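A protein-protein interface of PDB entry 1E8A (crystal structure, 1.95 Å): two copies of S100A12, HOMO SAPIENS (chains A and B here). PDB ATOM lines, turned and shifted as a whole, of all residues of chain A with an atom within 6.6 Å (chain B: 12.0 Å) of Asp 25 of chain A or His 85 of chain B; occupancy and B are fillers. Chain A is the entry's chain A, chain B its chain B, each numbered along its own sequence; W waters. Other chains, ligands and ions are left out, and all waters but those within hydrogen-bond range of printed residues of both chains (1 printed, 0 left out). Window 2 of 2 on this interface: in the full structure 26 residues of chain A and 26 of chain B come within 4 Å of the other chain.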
ATOM      1  N   LEU A   7      -8.889   4.499  16.812  1.00  0.00           N
ATOM      2  CA  LEU A   7      -9.196   4.064  15.493  1.00  0.00           C
ATOM      3  C   LEU A   7      -8.474   2.745  15.199  1.00  0.00           C
ATOM      4  O   LEU A   7      -9.101   1.820  14.677  1.00  0.00           O
ATOM      5  CB  LEU A   7      -8.875   5.120  14.453  1.00  0.00           C
ATOM      6  CG  LEU A   7      -9.690   6.403  14.563  1.00  0.00           C
ATOM      7  CD1 LEU A   7      -9.009   7.541  13.791  1.00  0.00           C
ATOM      8  CD2 LEU A   7     -11.138   6.234  14.077  1.00  0.00           C
ATOM      9  N   GLU A   8      -7.182   2.679  15.571  1.00  0.00           N
ATOM     10  CA  GLU A   8      -6.375   1.514  15.362  1.00  0.00           C
ATOM     11  C   GLU A   8      -6.947   0.369  16.181  1.00  0.00           C
ATOM     12  O   GLU A   8      -6.931  -0.766  15.723  1.00  0.00           O
ATOM     13  CB  GLU A   8      -4.952   1.774  15.800  1.00  0.00           C
ATOM     14  CG  GLU A   8      -4.118   0.499  15.895  1.00  0.00           C
ATOM     15  CD  GLU A   8      -3.944  -0.263  14.569  1.00  0.00           C
ATOM     16  OE1 GLU A   8      -4.232   0.312  13.478  1.00  0.00           O
ATOM     17  OE2 GLU A   8      -3.534  -1.488  14.624  1.00  0.00           O
ATOM     18  N   VAL A  11      -9.841  -1.131  14.264  1.00  0.00           N
ATOM     19  CA  VAL A  11      -9.349  -1.946  13.179  1.00  0.00           C
ATOM     20  C   VAL A  11      -8.799  -3.265  13.727  1.00  0.00           C
ATOM     21  O   VAL A  11      -9.055  -4.333  13.144  1.00  0.00           O
ATOM     22  CB  VAL A  11      -8.306  -1.247  12.312  1.00  0.00           C
ATOM     23  CG1 VAL A  11      -7.772  -2.188  11.207  1.00  0.00           C
ATOM     24  CG2 VAL A  11      -8.828   0.057  11.748  1.00  0.00           C
ATOM     25  N   PHE A  14     -11.652  -5.613  14.463  1.00  0.00           N
ATOM     26  CA  PHE A  14     -12.161  -6.136  13.258  1.00  0.00           C
ATOM     27  C   PHE A  14     -11.364  -7.375  12.879  1.00  0.00           C
ATOM     28  O   PHE A  14     -11.925  -8.422  12.590  1.00  0.00           O
ATOM     29  CB  PHE A  14     -12.128  -5.095  12.129  1.00  0.00           C
ATOM     30  CG  PHE A  14     -12.453  -5.664  10.768  1.00  0.00           C
ATOM     31  CD1 PHE A  14     -13.767  -5.766  10.332  1.00  0.00           C
ATOM     32  CD2 PHE A  14     -11.442  -6.100   9.902  1.00  0.00           C
ATOM     33  CE1 PHE A  14     -14.077  -6.301   9.121  1.00  0.00           C
ATOM     34  CE2 PHE A  14     -11.760  -6.606   8.655  1.00  0.00           C
ATOM     35  CZ  PHE A  14     -13.108  -6.721   8.257  1.00  0.00           C
ATOM     36  N   HIS A  15     -10.050  -7.259  12.870  1.00  0.00           N
ATOM     37  CA  HIS A  15      -9.242  -8.404  12.519  1.00  0.00           C
ATOM     38  C   HIS A  15      -9.235  -9.494  13.588  1.00  0.00           C
ATOM     39  O   HIS A  15      -9.079 -10.683  13.267  1.00  0.00           O
ATOM     40  CB  HIS A  15      -7.817  -7.982  12.185  1.00  0.00           C
ATOM     41  CG  HIS A  15      -7.700  -7.293  10.868  1.00  0.00           C
ATOM     42  ND1 HIS A  15      -7.575  -5.928  10.783  1.00  0.00           N
ATOM     43  CD2 HIS A  15      -8.059  -7.697   9.632  1.00  0.00           C
ATOM     44  CE1 HIS A  15      -7.575  -5.578   9.502  1.00  0.00           C
ATOM     45  NE2 HIS A  15      -7.758  -6.662   8.782  1.00  0.00           N
ATOM     46  N   SER A  18     -12.038 -11.177  12.052  1.00  0.00           N
ATOM     47  CA  SER A  18     -12.070 -11.505  10.630  1.00  0.00           C
ATOM     48  C   SER A  18     -11.087 -12.607  10.199  1.00  0.00           C
ATOM     49  O   SER A  18     -11.311 -13.305   9.174  1.00  0.00           O
ATOM     50  CB  SER A  18     -11.796 -10.286   9.751  1.00  0.00           C
ATOM     51  OG  SER A  18     -10.464  -9.777   9.890  1.00  0.00           O
ATOM     52  N   VAL A  19     -10.014 -12.779  10.954  1.00  0.00           N
ATOM     53  CA  VAL A  19      -9.046 -13.760  10.564  1.00  0.00           C
ATOM     54  C   VAL A  19      -9.445 -15.165  10.942  1.00  0.00           C
ATOM     55  O   VAL A  19      -8.775 -16.119  10.583  1.00  0.00           O
ATOM     56  CB  VAL A  19      -7.672 -13.499  11.150  1.00  0.00           C
ATOM     57  CG1 VAL A  19      -7.117 -12.052  10.784  1.00  0.00           C
ATOM     58  CG2 VAL A  19      -7.678 -13.715  12.644  1.00  0.00           C
ATOM     59  N   GLY A  22     -12.210 -18.530   6.994  1.00  0.00           N
ATOM     60  CA  GLY A  22     -12.268 -18.064   5.611  1.00  0.00           C
ATOM     61  C   GLY A  22     -11.353 -16.895   5.348  1.00  0.00           C
ATOM     62  O   GLY A  22     -10.229 -16.892   5.882  1.00  0.00           O
ATOM     63  N   HIS A  23     -11.763 -15.977   4.483  1.00  0.00           N
ATOM     64  CA  HIS A  23     -10.937 -14.800   4.145  1.00  0.00           C
ATOM     65  C   HIS A  23     -10.494 -14.041   5.412  1.00  0.00           C
ATOM     66  O   HIS A  23     -11.330 -13.790   6.286  1.00  0.00           O
ATOM     67  CB  HIS A  23     -11.697 -13.850   3.190  1.00  0.00           C
ATOM     68  CG  HIS A  23     -10.823 -12.790   2.576  1.00  0.00           C
ATOM     69  ND1 HIS A  23     -10.353 -12.857   1.264  1.00  0.00           N
ATOM     70  CD2 HIS A  23     -10.275 -11.669   3.113  1.00  0.00           C
ATOM     71  CE1 HIS A  23      -9.716 -11.727   0.987  1.00  0.00           C
ATOM     72  NE2 HIS A  23      -9.572 -11.039   2.113  1.00  0.00           N
ATOM     73  N   PHE A  24      -9.235 -13.596   5.446  1.00  0.00           N
ATOM     74  CA  PHE A  24      -8.668 -12.889   6.578  1.00  0.00           C
ATOM     75  C   PHE A  24      -9.201 -11.476   6.760  1.00  0.00           C
ATOM     76  O   PHE A  24      -9.096 -10.935   7.841  1.00  0.00           O
ATOM     77  CB  PHE A  24      -7.125 -12.786   6.520  1.00  0.00           C
ATOM     78  CG  PHE A  24      -6.396 -14.061   6.903  1.00  0.00           C
ATOM     79  CD1 PHE A  24      -7.072 -15.219   7.168  1.00  0.00           C
ATOM     80  CD2 PHE A  24      -5.018 -14.062   7.088  1.00  0.00           C
ATOM     81  CE1 PHE A  24      -6.391 -16.361   7.548  1.00  0.00           C
ATOM     82  CE2 PHE A  24      -4.355 -15.201   7.448  1.00  0.00           C
ATOM     83  CZ  PHE A  24      -5.054 -16.367   7.642  1.00  0.00           C
ATOM     84  N   ASP A  25      -9.733 -10.876   5.711  1.00  0.00           N
ATOM     85  CA  ASP A  25     -10.085  -9.448   5.733  1.00  0.00           C
ATOM     86  C   ASP A  25     -11.580  -9.228   5.597  1.00  0.00           C
ATOM     87  O   ASP A  25     -12.029  -8.132   5.300  1.00  0.00           O
ATOM     88  CB  ASP A  25      -9.393  -8.752   4.589  1.00  0.00           C
ATOM     89  CG  ASP A  25      -9.170  -7.213   4.818  1.00  0.00           C
ATOM     90  OD1 ASP A  25      -9.077  -6.711   5.957  1.00  0.00           O
ATOM     91  OD2 ASP A  25      -9.018  -6.417   3.858  1.00  0.00           O
ATOM     92  N   THR A  26     -12.378 -10.275   5.778  1.00  0.00           N
ATOM     93  CA  THR A  26     -13.811 -10.122   5.833  1.00  0.00           C
ATOM     94  C   THR A  26     -14.409 -10.999   6.931  1.00  0.00           C
ATOM     95  O   THR A  26     -13.843 -12.006   7.313  1.00  0.00           O
ATOM     96  CB  THR A  26     -14.523 -10.390   4.505  1.00  0.00           C
ATOM     97  OG1 THR A  26     -14.474 -11.781   4.184  1.00  0.00           O
ATOM     98  CG2 THR A  26     -13.835  -9.746   3.314  1.00  0.00           C
ATOM     99  N   LEU A  27     -15.547 -10.564   7.434  1.00  0.00           N
ATOM    100  CA  LEU A  27     -16.288 -11.240   8.500  1.00  0.00           C
ATOM    101  C   LEU A  27     -17.373 -12.087   7.914  1.00  0.00           C
ATOM    102  O   LEU A  27     -18.251 -11.598   7.183  1.00  0.00           O
ATOM    103  CB  LEU A  27     -16.944 -10.225   9.450  1.00  0.00           C
ATOM    104  CG  LEU A  27     -15.987  -9.297  10.190  1.00  0.00           C
ATOM    105  CD1 LEU A  27     -16.751  -8.107  10.724  1.00  0.00           C
ATOM    106  CD2 LEU A  27     -15.299 -10.005  11.341  1.00  0.00           C
ATOM    107  N   GLN A  67     -20.452 -11.866   3.306  1.00  0.00           N
ATOM    108  CA  GLN A  67     -19.314 -11.456   4.128  1.00  0.00           C
ATOM    109  C   GLN A  67     -19.488 -10.014   4.416  1.00  0.00           C
ATOM    110  O   GLN A  67     -20.068  -9.278   3.592  1.00  0.00           O
ATOM    111  CB  GLN A  67     -18.033 -11.536   3.336  1.00  0.00           C
ATOM    112  CG  GLN A  67     -17.761 -12.899   2.849  1.00  0.00           C
ATOM    113  CD  GLN A  67     -17.268 -13.776   3.976  1.00  0.00           C
ATOM    114  OE1 GLN A  67     -16.482 -13.317   4.814  1.00  0.00           O
ATOM    115  NE2 GLN A  67     -17.688 -15.019   3.996  1.00  0.00           N
ATOM    116  N   VAL A  68     -18.979  -9.581   5.573  1.00  0.00           N
ATOM    117  CA  VAL A  68     -18.902  -8.191   5.873  1.00  0.00           C
ATOM    118  C   VAL A  68     -17.467  -7.701   5.778  1.00  0.00           C
ATOM    119  O   VAL A  68     -16.585  -8.074   6.593  1.00  0.00           O
ATOM    120  CB  VAL A  68     -19.575  -7.871   7.221  1.00  0.00           C
ATOM    121  CG1 VAL A  68     -19.384  -6.400   7.532  1.00  0.00           C
ATOM    122  CG2 VAL A  68     -21.093  -8.268   7.212  1.00  0.00           C
ATOM    123  N   ASP A  69     -17.202  -6.927   4.717  1.00  0.00           N
ATOM    124  CA  ASP A  69     -15.866  -6.399   4.505  1.00  0.00           C
ATOM    125  C   ASP A  69     -15.644  -5.111   5.339  1.00  0.00           C
ATOM    126  O   ASP A  69     -16.554  -4.650   6.058  1.00  0.00           O
ATOM    127  CB  ASP A  69     -15.586  -6.164   3.021  1.00  0.00           C
ATOM    128  CG  ASP A  69     -16.416  -5.112   2.420  1.00  0.00           C
ATOM    129  OD1 ASP A  69     -16.815  -4.142   3.105  1.00  0.00           O
ATOM    130  OD2 ASP A  69     -16.683  -5.173   1.192  1.00  0.00           O
ATOM    131  N   PHE A  70     -14.430  -4.577   5.286  1.00  0.00           N
ATOM    132  CA  PHE A  70     -14.061  -3.541   6.216  1.00  0.00           C
ATOM    133  C   PHE A  70     -14.936  -2.321   5.975  1.00  0.00           C
ATOM    134  O   PHE A  70     -15.423  -1.711   6.893  1.00  0.00           O
ATOM    135  CB  PHE A  70     -12.533  -3.185   6.239  1.00  0.00           C
ATOM    136  CG  PHE A  70     -12.196  -2.215   7.317  1.00  0.00           C
ATOM    137  CD1 PHE A  70     -12.190  -2.631   8.668  1.00  0.00           C
ATOM    138  CD2 PHE A  70     -12.093  -0.878   7.054  1.00  0.00           C
ATOM    139  CE1 PHE A  70     -11.996  -1.733   9.682  1.00  0.00           C
ATOM    140  CE2 PHE A  70     -11.840   0.034   8.109  1.00  0.00           C
ATOM    141  CZ  PHE A  70     -11.814  -0.383   9.390  1.00  0.00           C
ATOM    142  N   GLN A  71     -15.124  -1.989   4.719  1.00  0.00           N
ATOM    143  CA  GLN A  71     -15.915  -0.851   4.333  1.00  0.00           C
ATOM    144  C   GLN A  71     -17.372  -1.004   4.789  1.00  0.00           C
ATOM    145  O   GLN A  71     -17.969  -0.079   5.316  1.00  0.00           O
ATOM    146  CB  GLN A  71     -15.808  -0.677   2.851  1.00  0.00           C
ATOM    147  CG  GLN A  71     -16.413   0.587   2.468  1.00  0.00           C
ATOM    148  CD  GLN A  71     -15.492   1.755   2.846  1.00  0.00           C
ATOM    149  OE1 GLN A  71     -14.255   1.579   2.923  1.00  0.00           O
ATOM    150  NE2 GLN A  71     -16.072   2.944   3.048  1.00  0.00           N
ATOM    151  N   LEU B  40      -5.417  14.081  14.304  1.00  0.00           N
ATOM    152  CA  LEU B  40      -5.371  13.327  13.055  1.00  0.00           C
ATOM    153  C   LEU B  40      -4.169  13.579  12.121  1.00  0.00           C
ATOM    154  O   LEU B  40      -4.161  13.182  10.956  1.00  0.00           O
ATOM    155  CB  LEU B  40      -6.698  13.597  12.356  1.00  0.00           C
ATOM    156  CG  LEU B  40      -7.839  12.574  12.399  1.00  0.00           C
ATOM    157  CD1 LEU B  40      -7.600  11.439  13.337  1.00  0.00           C
ATOM    158  CD2 LEU B  40      -9.307  13.139  12.426  1.00  0.00           C
ATOM    159  N   ASN B  42      -1.311  12.238  11.860  1.00  0.00           N
ATOM    160  CA  ASN B  42      -0.673  11.054  11.349  1.00  0.00           C
ATOM    161  C   ASN B  42      -1.634  10.278  10.471  1.00  0.00           C
ATOM    162  O   ASN B  42      -1.306   9.179  10.007  1.00  0.00           O
ATOM    163  CB  ASN B  42      -0.174  10.177  12.487  1.00  0.00           C
ATOM    164  CG  ASN B  42       0.716  10.951  13.449  1.00  0.00           C
ATOM    165  OD1 ASN B  42       1.705  11.533  13.020  1.00  0.00           O
ATOM    166  ND2 ASN B  42       0.338  11.007  14.735  1.00  0.00           N
ATOM    167  N   THR B  43      -2.804  10.852  10.217  1.00  0.00           N
ATOM    168  CA  THR B  43      -3.819  10.147   9.449  1.00  0.00           C
ATOM    169  C   THR B  43      -4.198  10.851   8.173  1.00  0.00           C
ATOM    170  O   THR B  43      -4.413  10.220   7.157  1.00  0.00           O
ATOM    171  CB  THR B  43      -5.069   9.980  10.283  1.00  0.00           C
ATOM    172  OG1 THR B  43      -4.745   9.340  11.519  1.00  0.00           O
ATOM    173  CG2 THR B  43      -6.071   9.025   9.583  1.00  0.00           C
ATOM    174  N   ILE B  44      -4.358  12.151   8.217  1.00  0.00           N
ATOM    175  CA  ILE B  44      -4.740  12.840   7.007  1.00  0.00           C
ATOM    176  C   ILE B  44      -3.609  13.718   6.600  1.00  0.00           C
ATOM    177  O   ILE B  44      -3.085  14.488   7.411  1.00  0.00           O
ATOM    178  CB  ILE B  44      -5.999  13.636   7.229  1.00  0.00           C
ATOM    179  CG1 ILE B  44      -7.158  12.694   7.593  1.00  0.00           C
ATOM    180  CG2 ILE B  44      -6.315  14.444   6.004  1.00  0.00           C
ATOM    181  CD1 ILE B  44      -8.481  13.406   7.916  1.00  0.00           C
ATOM    182  N   LEU B  76     -16.247  11.731   9.353  1.00  0.00           N
ATOM    183  CA  LEU B  76     -14.821  11.892   9.597  1.00  0.00           C
ATOM    184  C   LEU B  76     -14.214  10.608  10.188  1.00  0.00           C
ATOM    185  O   LEU B  76     -13.175  10.128   9.700  1.00  0.00           O
ATOM    186  CB  LEU B  76     -14.583  13.095  10.521  1.00  0.00           C
ATOM    187  CG  LEU B  76     -13.122  13.374  10.813  1.00  0.00           C
ATOM    188  CD1 LEU B  76     -12.272  13.615   9.557  1.00  0.00           C
ATOM    189  CD2 LEU B  76     -13.012  14.560  11.779  1.00  0.00           C
ATOM    190  N   VAL B  77     -14.864  10.024  11.189  1.00  0.00           N
ATOM    191  CA  VAL B  77     -14.392   8.740  11.717  1.00  0.00           C
ATOM    192  C   VAL B  77     -14.316   7.687  10.635  1.00  0.00           C
ATOM    193  O   VAL B  77     -13.344   6.927  10.607  1.00  0.00           O
ATOM    194  CB  VAL B  77     -15.221   8.214  12.905  1.00  0.00           C
ATOM    195  CG1 VAL B  77     -14.759   6.839  13.324  1.00  0.00           C
ATOM    196  CG2 VAL B  77     -15.140   9.119  14.069  1.00  0.00           C
ATOM    197  N   ALA B  78     -15.262   7.668   9.689  1.00  0.00           N
ATOM    198  CA  ALA B  78     -15.197   6.677   8.607  1.00  0.00           C
ATOM    199  C   ALA B  78     -13.982   6.885   7.702  1.00  0.00           C
ATOM    200  O   ALA B  78     -13.295   5.932   7.318  1.00  0.00           O
ATOM    201  CB  ALA B  78     -16.490   6.626   7.814  1.00  0.00           C
ATOM    202  N   ILE B  79     -13.696   8.131   7.379  1.00  0.00           N
ATOM    203  CA  ILE B  79     -12.523   8.472   6.585  1.00  0.00           C
ATOM    204  C   ILE B  79     -11.236   8.012   7.250  1.00  0.00           C
ATOM    205  O   ILE B  79     -10.356   7.415   6.602  1.00  0.00           O
ATOM    206  CB  ILE B  79     -12.519   9.989   6.356  1.00  0.00           C
ATOM    207  CG1 ILE B  79     -13.552  10.325   5.283  1.00  0.00           C
ATOM    208  CG2 ILE B  79     -11.116  10.493   5.993  1.00  0.00           C
ATOM    209  CD1 ILE B  79     -14.216  11.722   5.467  1.00  0.00           C
ATOM    210  N   ALA B  80     -11.146   8.249   8.547  1.00  0.00           N
ATOM    211  CA  ALA B  80      -9.977   7.927   9.327  1.00  0.00           C
ATOM    212  C   ALA B  80      -9.838   6.429   9.496  1.00  0.00           C
ATOM    213  O   ALA B  80      -8.743   5.892   9.493  1.00  0.00           O
ATOM    214  CB  ALA B  80     -10.073   8.592  10.681  1.00  0.00           C
ATOM    215  N   LEU B  81     -10.955   5.743   9.676  1.00  0.00           N
ATOM    216  CA  LEU B  81     -10.904   4.289   9.808  1.00  0.00           C
ATOM    217  C   LEU B  81     -10.345   3.637   8.564  1.00  0.00           C
ATOM    218  O   LEU B  81      -9.582   2.667   8.647  1.00  0.00           O
ATOM    219  CB  LEU B  81     -12.284   3.721  10.117  1.00  0.00           C
ATOM    220  CG  LEU B  81     -12.707   3.823  11.556  1.00  0.00           C
ATOM    221  CD1 LEU B  81     -14.196   3.420  11.750  1.00  0.00           C
ATOM    222  CD2 LEU B  81     -11.785   2.934  12.398  1.00  0.00           C
ATOM    223  N   LYS B  82     -10.754   4.122   7.407  1.00  0.00           N
ATOM    224  CA  LYS B  82     -10.283   3.552   6.165  1.00  0.00           C
ATOM    225  C   LYS B  82      -8.759   3.668   6.055  1.00  0.00           C
ATOM    226  O   LYS B  82      -8.058   2.712   5.608  1.00  0.00           O
ATOM    227  CB  LYS B  82     -10.980   4.220   4.993  1.00  0.00           C
ATOM    228  N   ALA B  83      -8.238   4.808   6.491  1.00  0.00           N
ATOM    229  CA  ALA B  83      -6.787   5.031   6.460  1.00  0.00           C
ATOM    230  C   ALA B  83      -6.031   4.070   7.420  1.00  0.00           C
ATOM    231  O   ALA B  83      -5.025   3.463   7.056  1.00  0.00           O
ATOM    232  CB  ALA B  83      -6.490   6.481   6.752  1.00  0.00           C
ATOM    233  N   ALA B  84      -6.544   3.846   8.609  1.00  0.00           N
ATOM    234  CA  ALA B  84      -5.876   2.967   9.551  1.00  0.00           C
ATOM    235  C   ALA B  84      -5.867   1.549   9.039  1.00  0.00           C
ATOM    236  O   ALA B  84      -4.844   0.830   9.059  1.00  0.00           O
ATOM    237  CB  ALA B  84      -6.575   3.061  10.892  1.00  0.00           C
ATOM    238  N   HIS B  85      -6.999   1.126   8.503  1.00  0.00           N
ATOM    239  CA  HIS B  85      -7.105  -0.217   7.975  1.00  0.00           C
ATOM    240  C   HIS B  85      -6.238  -0.581   6.791  1.00  0.00           C
ATOM    241  O   HIS B  85      -5.878  -1.769   6.613  1.00  0.00           O
ATOM    242  CB  HIS B  85      -8.559  -0.482   7.578  1.00  0.00           C
ATOM    243  CG  HIS B  85      -8.746  -1.780   6.867  1.00  0.00           C
ATOM    244  ND1 HIS B  85      -8.783  -1.884   5.496  1.00  0.00           N
ATOM    245  CD2 HIS B  85      -8.959  -3.030   7.342  1.00  0.00           C
ATOM    246  CE1 HIS B  85      -8.901  -3.152   5.165  1.00  0.00           C
ATOM    247  NE2 HIS B  85      -9.177  -3.839   6.259  1.00  0.00           N
ATOM    248  N   TYR B  86      -5.904   0.396   5.957  1.00  0.00           N
ATOM    249  CA  TYR B  86      -5.192   0.113   4.737  1.00  0.00           C
ATOM    250  C   TYR B  86      -3.956  -0.831   4.847  1.00  0.00           C
ATOM    251  O   TYR B  86      -2.997  -0.573   5.593  1.00  0.00           O
ATOM    252  CB  TYR B  86      -4.797   1.427   4.014  1.00  0.00           C
ATOM    253  CG  TYR B  86      -4.022   1.187   2.749  1.00  0.00           C
ATOM    254  N   HIS B  87      -4.007  -1.917   4.088  1.00  0.00           N
ATOM    255  CA  HIS B  87      -2.929  -2.883   4.047  1.00  0.00           C
ATOM    256  C   HIS B  87      -1.802  -2.360   3.153  1.00  0.00           C
ATOM    257  O   HIS B  87      -2.012  -1.974   1.997  1.00  0.00           O
ATOM    258  CB  HIS B  87      -3.444  -4.208   3.502  1.00  0.00           C
ATOM    259  CG  HIS B  87      -2.365  -5.205   3.238  1.00  0.00           C
ATOM    260  ND1 HIS B  87      -1.757  -5.336   2.014  1.00  0.00           N
ATOM    261  CD2 HIS B  87      -1.793  -6.122   4.046  1.00  0.00           C
ATOM    262  CE1 HIS B  87      -0.901  -6.341   2.064  1.00  0.00           C
ATOM    263  NE2 HIS B  87      -0.877  -6.805   3.302  1.00  0.00           N
ATOM    264  N   THR B  88      -0.596  -2.325   3.695  1.00  0.00           N
ATOM    265  CA  THR B  88       0.557  -1.931   2.883  1.00  0.00           C
ATOM    266  C   THR B  88       1.668  -2.961   2.949  1.00  0.00           C
ATOM    267  O   THR B  88       1.412  -4.112   3.263  1.00  0.00           O
ATOM    268  CB  THR B  88       1.102  -0.581   3.317  1.00  0.00           C
ATOM    269  OG1 THR B  88       2.221  -0.259   2.479  1.00  0.00           O
ATOM    270  CG2 THR B  88       1.681  -0.655   4.724  1.00  0.00           C
HETATM  271  O   HOH W   1      -5.636  -4.325   7.663  1.00  0.00           O
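Of the printed residues of chain B, Asp 25 of chain A touches His 85 (2.9 Å).
His 85 of chain B touches four residues of chain A.
Val 11 of chain A touches two residues of chain B.
His 15 of chain A touches one residue of chain B.
No residue of chain B comes within 4 Å of Ser 18 of chain A.
No residue of chain B comes within 4 Å of His 23 of chain A.
No residue of chain B comes within 4 Å of Phe 24 of chain A.
No residue of chain B comes within 4 Å of Leu 27 of chain A.
Asp 69 of chain A touches none of the printed residues of chain B.
Of the printed residues of chain B, Phe 70 of chain A touches Leu 81 and His 85.
Printed residues of chain A within 4 Å of Ala 80 of chain B: Leu 7 (3.5 Å).
Printed residues of chain A within 4 Å of Ala 84 of chain B: Val 11 (3.9 Å).
Of the printed residues of chain A, Leu 81 of chain B touches Leu 7 and Phe 70.
Of the printed residues of chain B, Leu 7 of chain A touches Val 77, Ala 80 and Leu 81.
Of the printed residues of chain A, Val 77 of chain B touches Leu 7 (3.7 Å).
Ile 44 of chain B touches none of the printed residues of chain A.
Ile 79 of chain B touches none of the printed residues of chain A.
The nearest residue of chain B that does not touch Asp 25 of chain A is His 87 of chain B (6.0 Å).
Water W1 bridges O of His 85 of chain B and NE2 of His 15 of chain A.
The side-chain carboxylate of Asp 25 of chain A sits at hydrogen-bond distance from a ring nitrogen (NE2) of His 85 of chain B (2.9 Å).
Hydrophobic or aromatic side chains of chain B that line the printed part of chain A: Val 77, Ala 80, Leu 81, Ala 84 and His 85.
Along chain B the printed residues that touch a printed residue of chain A span positions 77 to 85.
Printed residues of chain A that touch a printed residue of chain B: Leu 7, Val 11, His 15, Asp 25 and Phe 70.
Hydrophobic or aromatic side chains of chain A that line the printed part of chain B: Leu 7, Val 11, His 15 and Phe 70.
Along chain A the printed residues that touch a printed residue of chain B span positions 7 to 70.
Among the printed residues, no Asp or Glu carboxylate lies within 4 Å of a Lys or Arg side-chain nitrogen of the other chain.
O of Val 11 of chain A lies within hydrogen-bond range of ND1 of His 15 of chain A (3.2 Å).
NE2 of His 15 of chain A sits at hydrogen-bond distance from OD1 of Asp 25 of chain A.
CD2 of Leu 7 of chain A touches CG1 of Val 77 of chain B, at 3.7 Å.
CD1 of Leu 7 of chain A touches CB of Ala 80 of chain B, at 3.5 Å.
O of Leu 7 of chain A touches CD2 of Leu 81 of chain B, 3.7 Å away.
Ala 84 of chain B touches Val 11 of chain A (CB to CG2, 3.9 Å).
Val 11 of chain A touches His 85 of chain B (CG1 to CA, 3.8 Å).
His 15 of chain A touches His 85 of chain B (CE1 to CD2, 3.6 Å).
CE2 of Phe 70 of chain A touches O of Leu 81 of chain B (3.5 Å).
Phe 70 of chain A touches His 85 of chain B (CG to CD2, 3.3 Å).
No position is printed for both chains.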
